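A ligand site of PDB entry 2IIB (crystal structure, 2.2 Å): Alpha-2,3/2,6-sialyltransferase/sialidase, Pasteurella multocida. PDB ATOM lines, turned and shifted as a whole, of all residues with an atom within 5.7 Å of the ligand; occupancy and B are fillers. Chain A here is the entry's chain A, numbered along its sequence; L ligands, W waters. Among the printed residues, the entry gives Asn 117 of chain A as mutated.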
ATOM      1  N   SER A  12      20.791   9.983  22.678  1.00  0.00           N
ATOM      2  CA  SER A  12      21.114   9.084  21.579  1.00  0.00           C
ATOM      3  C   SER A  12      20.656   7.654  21.811  1.00  0.00           C
ATOM      4  O   SER A  12      19.913   7.108  20.998  1.00  0.00           O
ATOM      5  CB  SER A  12      22.625   9.099  21.311  1.00  0.00           C
ATOM      6  OG  SER A  12      23.062  10.386  20.906  1.00  0.00           O
ATOM      7  N   LEU A  13      21.116   7.039  22.905  1.00  0.00           N
ATOM      8  CA  LEU A  13      20.899   5.602  23.119  1.00  0.00           C
ATOM      9  C   LEU A  13      19.435   5.216  23.301  1.00  0.00           C
ATOM     10  O   LEU A  13      19.005   4.203  22.752  1.00  0.00           O
ATOM     11  CB  LEU A  13      21.747   5.093  24.306  1.00  0.00           C
ATOM     12  CG  LEU A  13      21.798   3.596  24.617  1.00  0.00           C
ATOM     13  CD1 LEU A  13      22.118   2.740  23.389  1.00  0.00           C
ATOM     14  CD2 LEU A  13      22.810   3.327  25.734  1.00  0.00           C
ATOM     15  N   LEU A  16      17.810   5.211  19.913  1.00  0.00           N
ATOM     16  CA  LEU A  16      18.230   4.085  19.087  1.00  0.00           C
ATOM     17  C   LEU A  16      17.437   2.814  19.433  1.00  0.00           C
ATOM     18  O   LEU A  16      17.011   2.082  18.530  1.00  0.00           O
ATOM     19  CB  LEU A  16      19.748   3.836  19.223  1.00  0.00           C
ATOM     20  CG  LEU A  16      20.355   2.701  18.401  1.00  0.00           C
ATOM     21  CD1 LEU A  16      20.510   3.140  16.953  1.00  0.00           C
ATOM     22  CD2 LEU A  16      21.697   2.246  18.987  1.00  0.00           C
ATOM     23  N   ARG A  39      17.478  13.654  18.088  1.00  0.00           N
ATOM     24  CA  ARG A  39      18.679  13.344  17.297  1.00  0.00           C
ATOM     25  C   ARG A  39      18.353  12.617  15.989  1.00  0.00           C
ATOM     26  O   ARG A  39      19.228  12.422  15.137  1.00  0.00           O
ATOM     27  CB  ARG A  39      19.733  12.629  18.159  1.00  0.00           C
ATOM     28  CG  ARG A  39      20.158  13.446  19.428  1.00  0.00           C
ATOM     29  CD  ARG A  39      21.502  13.029  20.098  1.00  0.00           C
ATOM     30  NE  ARG A  39      21.678  13.753  21.379  1.00  0.00           N
ATOM     31  CZ  ARG A  39      22.528  13.439  22.374  1.00  0.00           C
ATOM     32  NH1 ARG A  39      23.338  12.375  22.298  1.00  0.00           N
ATOM     33  NH2 ARG A  39      22.564  14.199  23.472  1.00  0.00           N
ATOM     34  N   ASN A 117      19.866   6.672  29.087  1.00  0.00           N
ATOM     35  CA  ASN A 117      20.647   7.667  28.384  1.00  0.00           C
ATOM     36  C   ASN A 117      22.005   7.044  28.028  1.00  0.00           C
ATOM     37  O   ASN A 117      22.527   7.215  26.913  1.00  0.00           O
ATOM     38  CB  ASN A 117      20.849   8.866  29.303  1.00  0.00           C
ATOM     39  CG  ASN A 117      21.370  10.085  28.573  1.00  0.00           C
ATOM     40  OD1 ASN A 117      20.602  10.981  28.261  1.00  0.00           O
ATOM     41  ND2 ASN A 117      22.672  10.117  28.304  1.00  0.00           N
ATOM     42  N   GLY A 118      22.575   6.322  28.994  1.00  0.00           N
ATOM     43  CA  GLY A 118      23.811   5.570  28.769  1.00  0.00           C
ATOM     44  C   GLY A 118      24.607   5.408  30.037  1.00  0.00           C
ATOM     45  O   GLY A 118      24.074   4.919  31.030  1.00  0.00           O
ATOM     46  N   SER A 119      25.868   5.845  29.993  1.00  0.00           N
ATOM     47  CA  SER A 119      26.742   5.857  31.163  1.00  0.00           C
ATOM     48  C   SER A 119      26.265   6.797  32.274  1.00  0.00           C
ATOM     49  O   SER A 119      26.560   6.573  33.448  1.00  0.00           O
ATOM     50  CB  SER A 119      28.152   6.296  30.744  1.00  0.00           C
ATOM     51  OG  SER A 119      28.166   7.678  30.435  1.00  0.00           O
ATOM     52  N   THR A 241      36.935   6.801  18.575  1.00  0.00           N
ATOM     53  CA  THR A 241      35.617   7.274  18.939  1.00  0.00           C
ATOM     54  C   THR A 241      35.719   8.646  19.620  1.00  0.00           C
ATOM     55  O   THR A 241      36.558   8.853  20.485  1.00  0.00           O
ATOM     56  CB  THR A 241      34.889   6.255  19.838  1.00  0.00           C
ATOM     57  OG1 THR A 241      35.555   6.168  21.113  1.00  0.00           O
ATOM     58  CG2 THR A 241      34.870   4.864  19.187  1.00  0.00           C
ATOM     59  N   GLY A 242      34.857   9.556  19.203  1.00  0.00           N
ATOM     60  CA  GLY A 242      34.848  10.890  19.759  1.00  0.00           C
ATOM     61  C   GLY A 242      33.889  11.055  20.931  1.00  0.00           C
ATOM     62  O   GLY A 242      33.072  10.168  21.227  1.00  0.00           O
ATOM     63  N   THR A 243      34.020  12.194  21.600  1.00  0.00           N
ATOM     64  CA  THR A 243      33.125  12.545  22.689  1.00  0.00           C
ATOM     65  C   THR A 243      32.595  13.944  22.424  1.00  0.00           C
ATOM     66  O   THR A 243      32.863  14.548  21.370  1.00  0.00           O
ATOM     67  CB  THR A 243      33.838  12.468  24.066  1.00  0.00           C
ATOM     68  OG1 THR A 243      32.862  12.589  25.110  1.00  0.00           O
ATOM     69  CG2 THR A 243      34.916  13.571  24.210  1.00  0.00           C
ATOM     70  N   THR A 244      31.807  14.449  23.371  1.00  0.00           N
ATOM     71  CA  THR A 244      31.364  15.815  23.290  1.00  0.00           C
ATOM     72  C   THR A 244      31.326  16.411  24.686  1.00  0.00           C
ATOM     73  O   THR A 244      31.516  15.718  25.680  1.00  0.00           O
ATOM     74  CB  THR A 244      29.999  15.944  22.530  1.00  0.00           C
ATOM     75  OG1 THR A 244      29.719  17.324  22.273  1.00  0.00           O
ATOM     76  CG2 THR A 244      28.860  15.320  23.325  1.00  0.00           C
ATOM     77  N   LYS A 285      34.687   7.758  14.407  1.00  0.00           N
ATOM     78  CA  LYS A 285      33.282   7.719  14.775  1.00  0.00           C
ATOM     79  C   LYS A 285      33.055   8.850  15.783  1.00  0.00           C
ATOM     80  O   LYS A 285      33.212   8.670  17.003  1.00  0.00           O
ATOM     81  CB  LYS A 285      32.909   6.333  15.336  1.00  0.00           C
ATOM     82  CG  LYS A 285      31.479   6.150  15.900  1.00  0.00           C
ATOM     83  CD  LYS A 285      30.395   6.212  14.808  1.00  0.00           C
ATOM     84  CE  LYS A 285      29.848   7.605  14.605  1.00  0.00           C
ATOM     85  NZ  LYS A 285      28.898   7.954  15.716  1.00  0.00           N
ATOM     86  N   GLY A 286      32.736  10.033  15.259  1.00  0.00           N
ATOM     87  CA  GLY A 286      32.471  11.191  16.104  1.00  0.00           C
ATOM     88  C   GLY A 286      31.256  10.976  16.990  1.00  0.00           C
ATOM     89  O   GLY A 286      30.398  10.146  16.681  1.00  0.00           O
ATOM     90  N   HIS A 287      31.191  11.721  18.096  1.00  0.00           N
ATOM     91  CA  HIS A 287      29.994  11.753  18.914  1.00  0.00           C
ATOM     92  C   HIS A 287      28.868  12.394  18.093  1.00  0.00           C
ATOM     93  O   HIS A 287      29.109  13.407  17.403  1.00  0.00           O
ATOM     94  CB  HIS A 287      30.214  12.552  20.204  1.00  0.00           C
ATOM     95  CG  HIS A 287      29.124  12.349  21.225  1.00  0.00           C
ATOM     96  ND1 HIS A 287      27.889  12.945  21.125  1.00  0.00           N
ATOM     97  CD2 HIS A 287      29.091  11.609  22.360  1.00  0.00           C
ATOM     98  CE1 HIS A 287      27.140  12.581  22.160  1.00  0.00           C
ATOM     99  NE2 HIS A 287      27.847  11.765  22.924  1.00  0.00           N
ATOM    100  N   PRO A 288      27.649  11.829  18.180  1.00  0.00           N
ATOM    101  CA  PRO A 288      26.468  12.401  17.506  1.00  0.00           C
ATOM    102  C   PRO A 288      26.291  13.909  17.697  1.00  0.00           C
ATOM    103  O   PRO A 288      25.768  14.565  16.801  1.00  0.00           O
ATOM    104  CB  PRO A 288      25.317  11.638  18.138  1.00  0.00           C
ATOM    105  CG  PRO A 288      25.895  10.295  18.417  1.00  0.00           C
ATOM    106  CD  PRO A 288      27.303  10.577  18.877  1.00  0.00           C
ATOM    107  N   ALA A 309      28.636  10.865  12.068  1.00  0.00           N
ATOM    108  CA  ALA A 309      28.485  10.990  13.515  1.00  0.00           C
ATOM    109  C   ALA A 309      27.137  10.558  14.090  1.00  0.00           C
ATOM    110  O   ALA A 309      27.094  10.030  15.194  1.00  0.00           O
ATOM    111  CB  ALA A 309      28.806  12.432  13.963  1.00  0.00           C
ATOM    112  N   ILE A 311      25.349   8.084  13.196  1.00  0.00           N
ATOM    113  CA  ILE A 311      25.234   6.628  13.191  1.00  0.00           C
ATOM    114  C   ILE A 311      25.750   6.098  14.524  1.00  0.00           C
ATOM    115  O   ILE A 311      26.944   6.173  14.815  1.00  0.00           O
ATOM    116  CB  ILE A 311      25.999   5.979  12.006  1.00  0.00           C
ATOM    117  CG1 ILE A 311      25.399   6.471  10.668  1.00  0.00           C
ATOM    118  CG2 ILE A 311      25.975   4.430  12.096  1.00  0.00           C
ATOM    119  CD1 ILE A 311      26.223   6.097   9.446  1.00  0.00           C
ATOM    120  N   SER A 312      24.840   5.558  15.326  1.00  0.00           N
ATOM    121  CA  SER A 312      25.230   4.970  16.611  1.00  0.00           C
ATOM    122  C   SER A 312      26.221   3.832  16.441  1.00  0.00           C
ATOM    123  O   SER A 312      25.997   2.905  15.652  1.00  0.00           O
ATOM    124  CB  SER A 312      24.011   4.488  17.393  1.00  0.00           C
ATOM    125  OG  SER A 312      23.347   5.592  17.981  1.00  0.00           O
ATOM    126  N   PHE A 313      27.307   3.902  17.210  1.00  0.00           N
ATOM    127  CA  PHE A 313      28.361   2.886  17.155  1.00  0.00           C
ATOM    128  C   PHE A 313      27.788   1.466  17.214  1.00  0.00           C
ATOM    129  O   PHE A 313      28.278   0.566  16.526  1.00  0.00           O
ATOM    130  CB  PHE A 313      29.386   3.089  18.276  1.00  0.00           C
ATOM    131  CG  PHE A 313      30.469   2.038  18.298  1.00  0.00           C
ATOM    132  CD1 PHE A 313      30.258   0.797  18.890  1.00  0.00           C
ATOM    133  CD2 PHE A 313      31.691   2.295  17.708  1.00  0.00           C
ATOM    134  CE1 PHE A 313      31.243  -0.171  18.892  1.00  0.00           C
ATOM    135  CE2 PHE A 313      32.696   1.331  17.713  1.00  0.00           C
ATOM    136  CZ  PHE A 313      32.481   0.109  18.298  1.00  0.00           C
ATOM    137  N   GLU A 314      26.741   1.285  18.015  1.00  0.00           N
ATOM    138  CA  GLU A 314      26.168  -0.043  18.260  1.00  0.00           C
ATOM    139  C   GLU A 314      25.564  -0.704  17.009  1.00  0.00           C
ATOM    140  O   GLU A 314      25.360  -1.918  16.981  1.00  0.00           O
ATOM    141  CB  GLU A 314      25.144   0.005  19.401  1.00  0.00           C
ATOM    142  CG  GLU A 314      25.717   0.408  20.762  1.00  0.00           C
ATOM    143  CD  GLU A 314      25.740   1.923  20.998  1.00  0.00           C
ATOM    144  OE1 GLU A 314      25.997   2.333  22.152  1.00  0.00           O
ATOM    145  OE2 GLU A 314      25.489   2.690  20.036  1.00  0.00           O
ATOM    146  N   ALA A 330      35.954   7.763  27.087  1.00  0.00           N
ATOM    147  CA  ALA A 330      34.905   6.986  27.752  1.00  0.00           C
ATOM    148  C   ALA A 330      33.539   7.341  27.201  1.00  0.00           C
ATOM    149  O   ALA A 330      33.178   8.537  27.078  1.00  0.00           O
ATOM    150  CB  ALA A 330      34.963   7.209  29.261  1.00  0.00           C
ATOM    151  N   SER A 331      32.791   6.311  26.842  1.00  0.00           N
ATOM    152  CA  SER A 331      31.512   6.471  26.163  1.00  0.00           C
ATOM    153  C   SER A 331      30.599   5.298  26.480  1.00  0.00           C
ATOM    154  O   SER A 331      31.061   4.192  26.797  1.00  0.00           O
ATOM    155  CB  SER A 331      31.722   6.547  24.648  1.00  0.00           C
ATOM    156  OG  SER A 331      30.454   6.647  23.977  1.00  0.00           O
ATOM    157  N   SER A 332      29.288   5.564  26.387  1.00  0.00           N
ATOM    158  CA  SER A 332      28.258   4.560  26.530  1.00  0.00           C
ATOM    159  C   SER A 332      28.488   3.376  25.591  1.00  0.00           C
ATOM    160  O   SER A 332      28.163   2.235  25.922  1.00  0.00           O
ATOM    161  CB  SER A 332      26.885   5.175  26.262  1.00  0.00           C
ATOM    162  OG  SER A 332      26.592   6.141  27.252  1.00  0.00           O
ATOM    163  N   LEU A 333      29.063   3.667  24.419  1.00  0.00           N
ATOM    164  CA  LEU A 333      29.311   2.640  23.396  1.00  0.00           C
ATOM    165  C   LEU A 333      30.235   1.518  23.917  1.00  0.00           C
ATOM    166  O   LEU A 333      30.138   0.396  23.450  1.00  0.00           O
ATOM    167  CB  LEU A 333      29.869   3.274  22.112  1.00  0.00           C
ATOM    168  CG  LEU A 333      31.328   3.747  22.073  1.00  0.00           C
ATOM    169  CD1 LEU A 333      32.274   2.593  21.710  1.00  0.00           C
ATOM    170  CD2 LEU A 333      31.488   4.919  21.091  1.00  0.00           C
ATOM    171  N   TYR A 364      32.831   7.838  37.078  1.00  0.00           N
ATOM    172  CA  TYR A 364      32.822   7.165  35.770  1.00  0.00           C
ATOM    173  C   TYR A 364      33.913   6.072  35.721  1.00  0.00           C
ATOM    174  O   TYR A 364      33.636   4.930  35.322  1.00  0.00           O
ATOM    175  CB  TYR A 364      33.004   8.176  34.637  1.00  0.00           C
ATOM    176  CG  TYR A 364      32.502   7.739  33.266  1.00  0.00           C
ATOM    177  CD1 TYR A 364      32.362   8.661  32.227  1.00  0.00           C
ATOM    178  CD2 TYR A 364      32.146   6.404  33.003  1.00  0.00           C
ATOM    179  CE1 TYR A 364      31.916   8.279  30.966  1.00  0.00           C
ATOM    180  CE2 TYR A 364      31.702   6.013  31.746  1.00  0.00           C
ATOM    181  CZ  TYR A 364      31.588   6.946  30.729  1.00  0.00           C
ATOM    182  OH  TYR A 364      31.142   6.558  29.481  1.00  0.00           O
HETATM  183  O1  LIG L   1      29.490   9.004  24.520  1.00  0.00           O
HETATM  184  P1  LIG L   1      27.991   8.873  25.056  1.00  0.00           P
HETATM  185  O2  LIG L   1      27.292  10.293  25.050  1.00  0.00           O
HETATM  186  O3  LIG L   1      27.926   8.212  26.490  1.00  0.00           O
HETATM  187  O4  LIG L   1      27.251   7.885  24.053  1.00  0.00           O
HETATM  188  C1  LIG L   1      25.848   7.731  24.095  1.00  0.00           C
HETATM  189  C2  LIG L   1      25.471   7.035  22.811  1.00  0.00           C
HETATM  190  O5  LIG L   1      25.721   7.813  21.610  1.00  0.00           O
HETATM  191  C3  LIG L   1      26.060   5.654  22.564  1.00  0.00           C
HETATM  192  O6  LIG L   1      25.467   4.516  23.152  1.00  0.00           O
HETATM  193  C4  LIG L   1      26.354   5.599  21.092  1.00  0.00           C
HETATM  194  O7  LIG L   1      25.168   5.055  20.525  1.00  0.00           O
HETATM  195  C5  LIG L   1      26.277   7.001  20.560  1.00  0.00           C
HETATM  196  N1  LIG L   1      27.677   7.362  20.268  1.00  0.00           N
HETATM  197  C6  LIG L   1      28.220   7.025  19.016  1.00  0.00           C
HETATM  198  N2  LIG L   1      29.518   7.349  18.695  1.00  0.00           N
HETATM  199  C7  LIG L   1      30.302   7.992  19.593  1.00  0.00           C
HETATM  200  C8  LIG L   1      29.791   8.332  20.839  1.00  0.00           C
HETATM  201  C9  LIG L   1      28.472   8.014  21.155  1.00  0.00           C
HETATM  202  O8  LIG L   1      27.486   6.430  18.208  1.00  0.00           O
HETATM  203  N3  LIG L   1      31.589   8.310  19.293  1.00  0.00           N
HETATM  204  O   HOH W   1      22.609   8.809  24.824  1.00  0.00           O
HETATM  205  O   HOH W   2      24.698  10.762  25.088  1.00  0.00           O
HETATM  206  O   HOH W   3      27.866  12.080  27.050  1.00  0.00           O
HETATM  207  O   HOH W   4      29.707   8.685  28.453  1.00  0.00           O
HETATM  208  O   HOH W   5      31.692  10.117  25.394  1.00  0.00           O
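An oxygen (O7) of the ligand lies within hydrogen-bond range of the side-chain carboxylate (OE2) of Glu 314, at 2.4 Å. N of Ser 332 lies within hydrogen-bond range of O3 of the ligand (3.0 Å). An oxygen (O3) of the ligand lies within hydrogen-bond range of the side-chain hydroxyl of Ser 332. An oxygen (O1) of the ligand sits at hydrogen-bond distance from the side-chain hydroxyl (OG) of Ser 331, 2.6 Å away. O2 of the ligand is in hydrogen-bond range of NE2 of His 287 (2.6 Å). The backbone NH (N) of Phe 313 lies within hydrogen-bond range of an oxygen (O8) of the ligand (2.7 Å). O of Lys 285 is in hydrogen-bond range of N3 of the ligand (2.8 Å). The side-chain amino group (NZ) of Lys 285 is in hydrogen-bond range of a nitrogen (N2) of the ligand (3.1 Å). N3 of the ligand is in hydrogen-bond range of O of Gly 242 (3.1 Å). The side-chain hydroxyl of Ser 312 lies within hydrogen-bond range of an oxygen (O7) of the ligand, at 3.2 Å. O of Gly 286 lies within hydrogen-bond range of N3 of the ligand (3.4 Å).
N of Ser 119 lies within hydrogen-bond range of OG of Ser 332, at 2.9 Å. The backbone NH (N) of Leu 333 lies close to the side-chain hydroxyl (OG) of Ser 331, 3.3 Å away. OH of Tyr 364 is in hydrogen-bond range of N of Ser 331 (3.1 Å). N of Gly 242 sits at hydrogen-bond distance from O of Lys 285 (2.9 Å). The side-chain amino group (NZ) of Lys 285 is in hydrogen-bond range of the backbone carbonyl oxygen (O) of Ile 311 (2.8 Å). NZ of Lys 285 sits at hydrogen-bond distance from O of Ala 309, at 2.8 Å. The side-chain hydroxyl (OG) of Ser 12 is in hydrogen-bond range of the guanidinium group (NH1) of Arg 39 (2.4 Å). The side-chain hydroxyl (OG) of Ser 119 lies close to the side-chain hydroxyl (OH) of Tyr 364, at 3.3 Å.
O8 of the ligand sits close to O of Ile 311 (3.4 Å). Merely in contact with the ligand: Ser 12 (3.4 Å), Leu 13 (3.8 Å), Ser 119 (3.99 Å), Thr 241 (3.9 Å), Pro 288 (3.5 Å) and Leu 333 (3.6 Å). Hydrophobic or aromatic side chains that line the ligand: Leu 13, His 287, Pro 288, Phe 313 and Leu 333. Of the 25 residues printed, 16 come within 4 Å of the ligand. The nearest printed residue that does not touch the ligand is Asn 117 (4.4 Å).
Water W5 lies within hydrogen-bond range of an oxygen (O1) of the ligand, the backbone carbonyl oxygen of Ala 330 and the side-chain hydroxyl of Thr 243. Water W2 bridges O2 of the ligand (2.6 Å) and NH1 of Arg 39 (3.5 Å). Water W4 lies within hydrogen-bond range of an oxygen (O3) of the ligand (2.7 Å), the side-chain hydroxyl of Ser 119 (2.7 Å) and the side-chain hydroxyl of Tyr 364 (2.8 Å). Water W1 lies within hydrogen-bond range of the backbone carbonyl oxygen (O) of Asn 117 (2.6 Å), the backbone NH (N) of Leu 13 (3.0 Å) and the backbone NH (N) of Ser 12 (3.0 Å).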
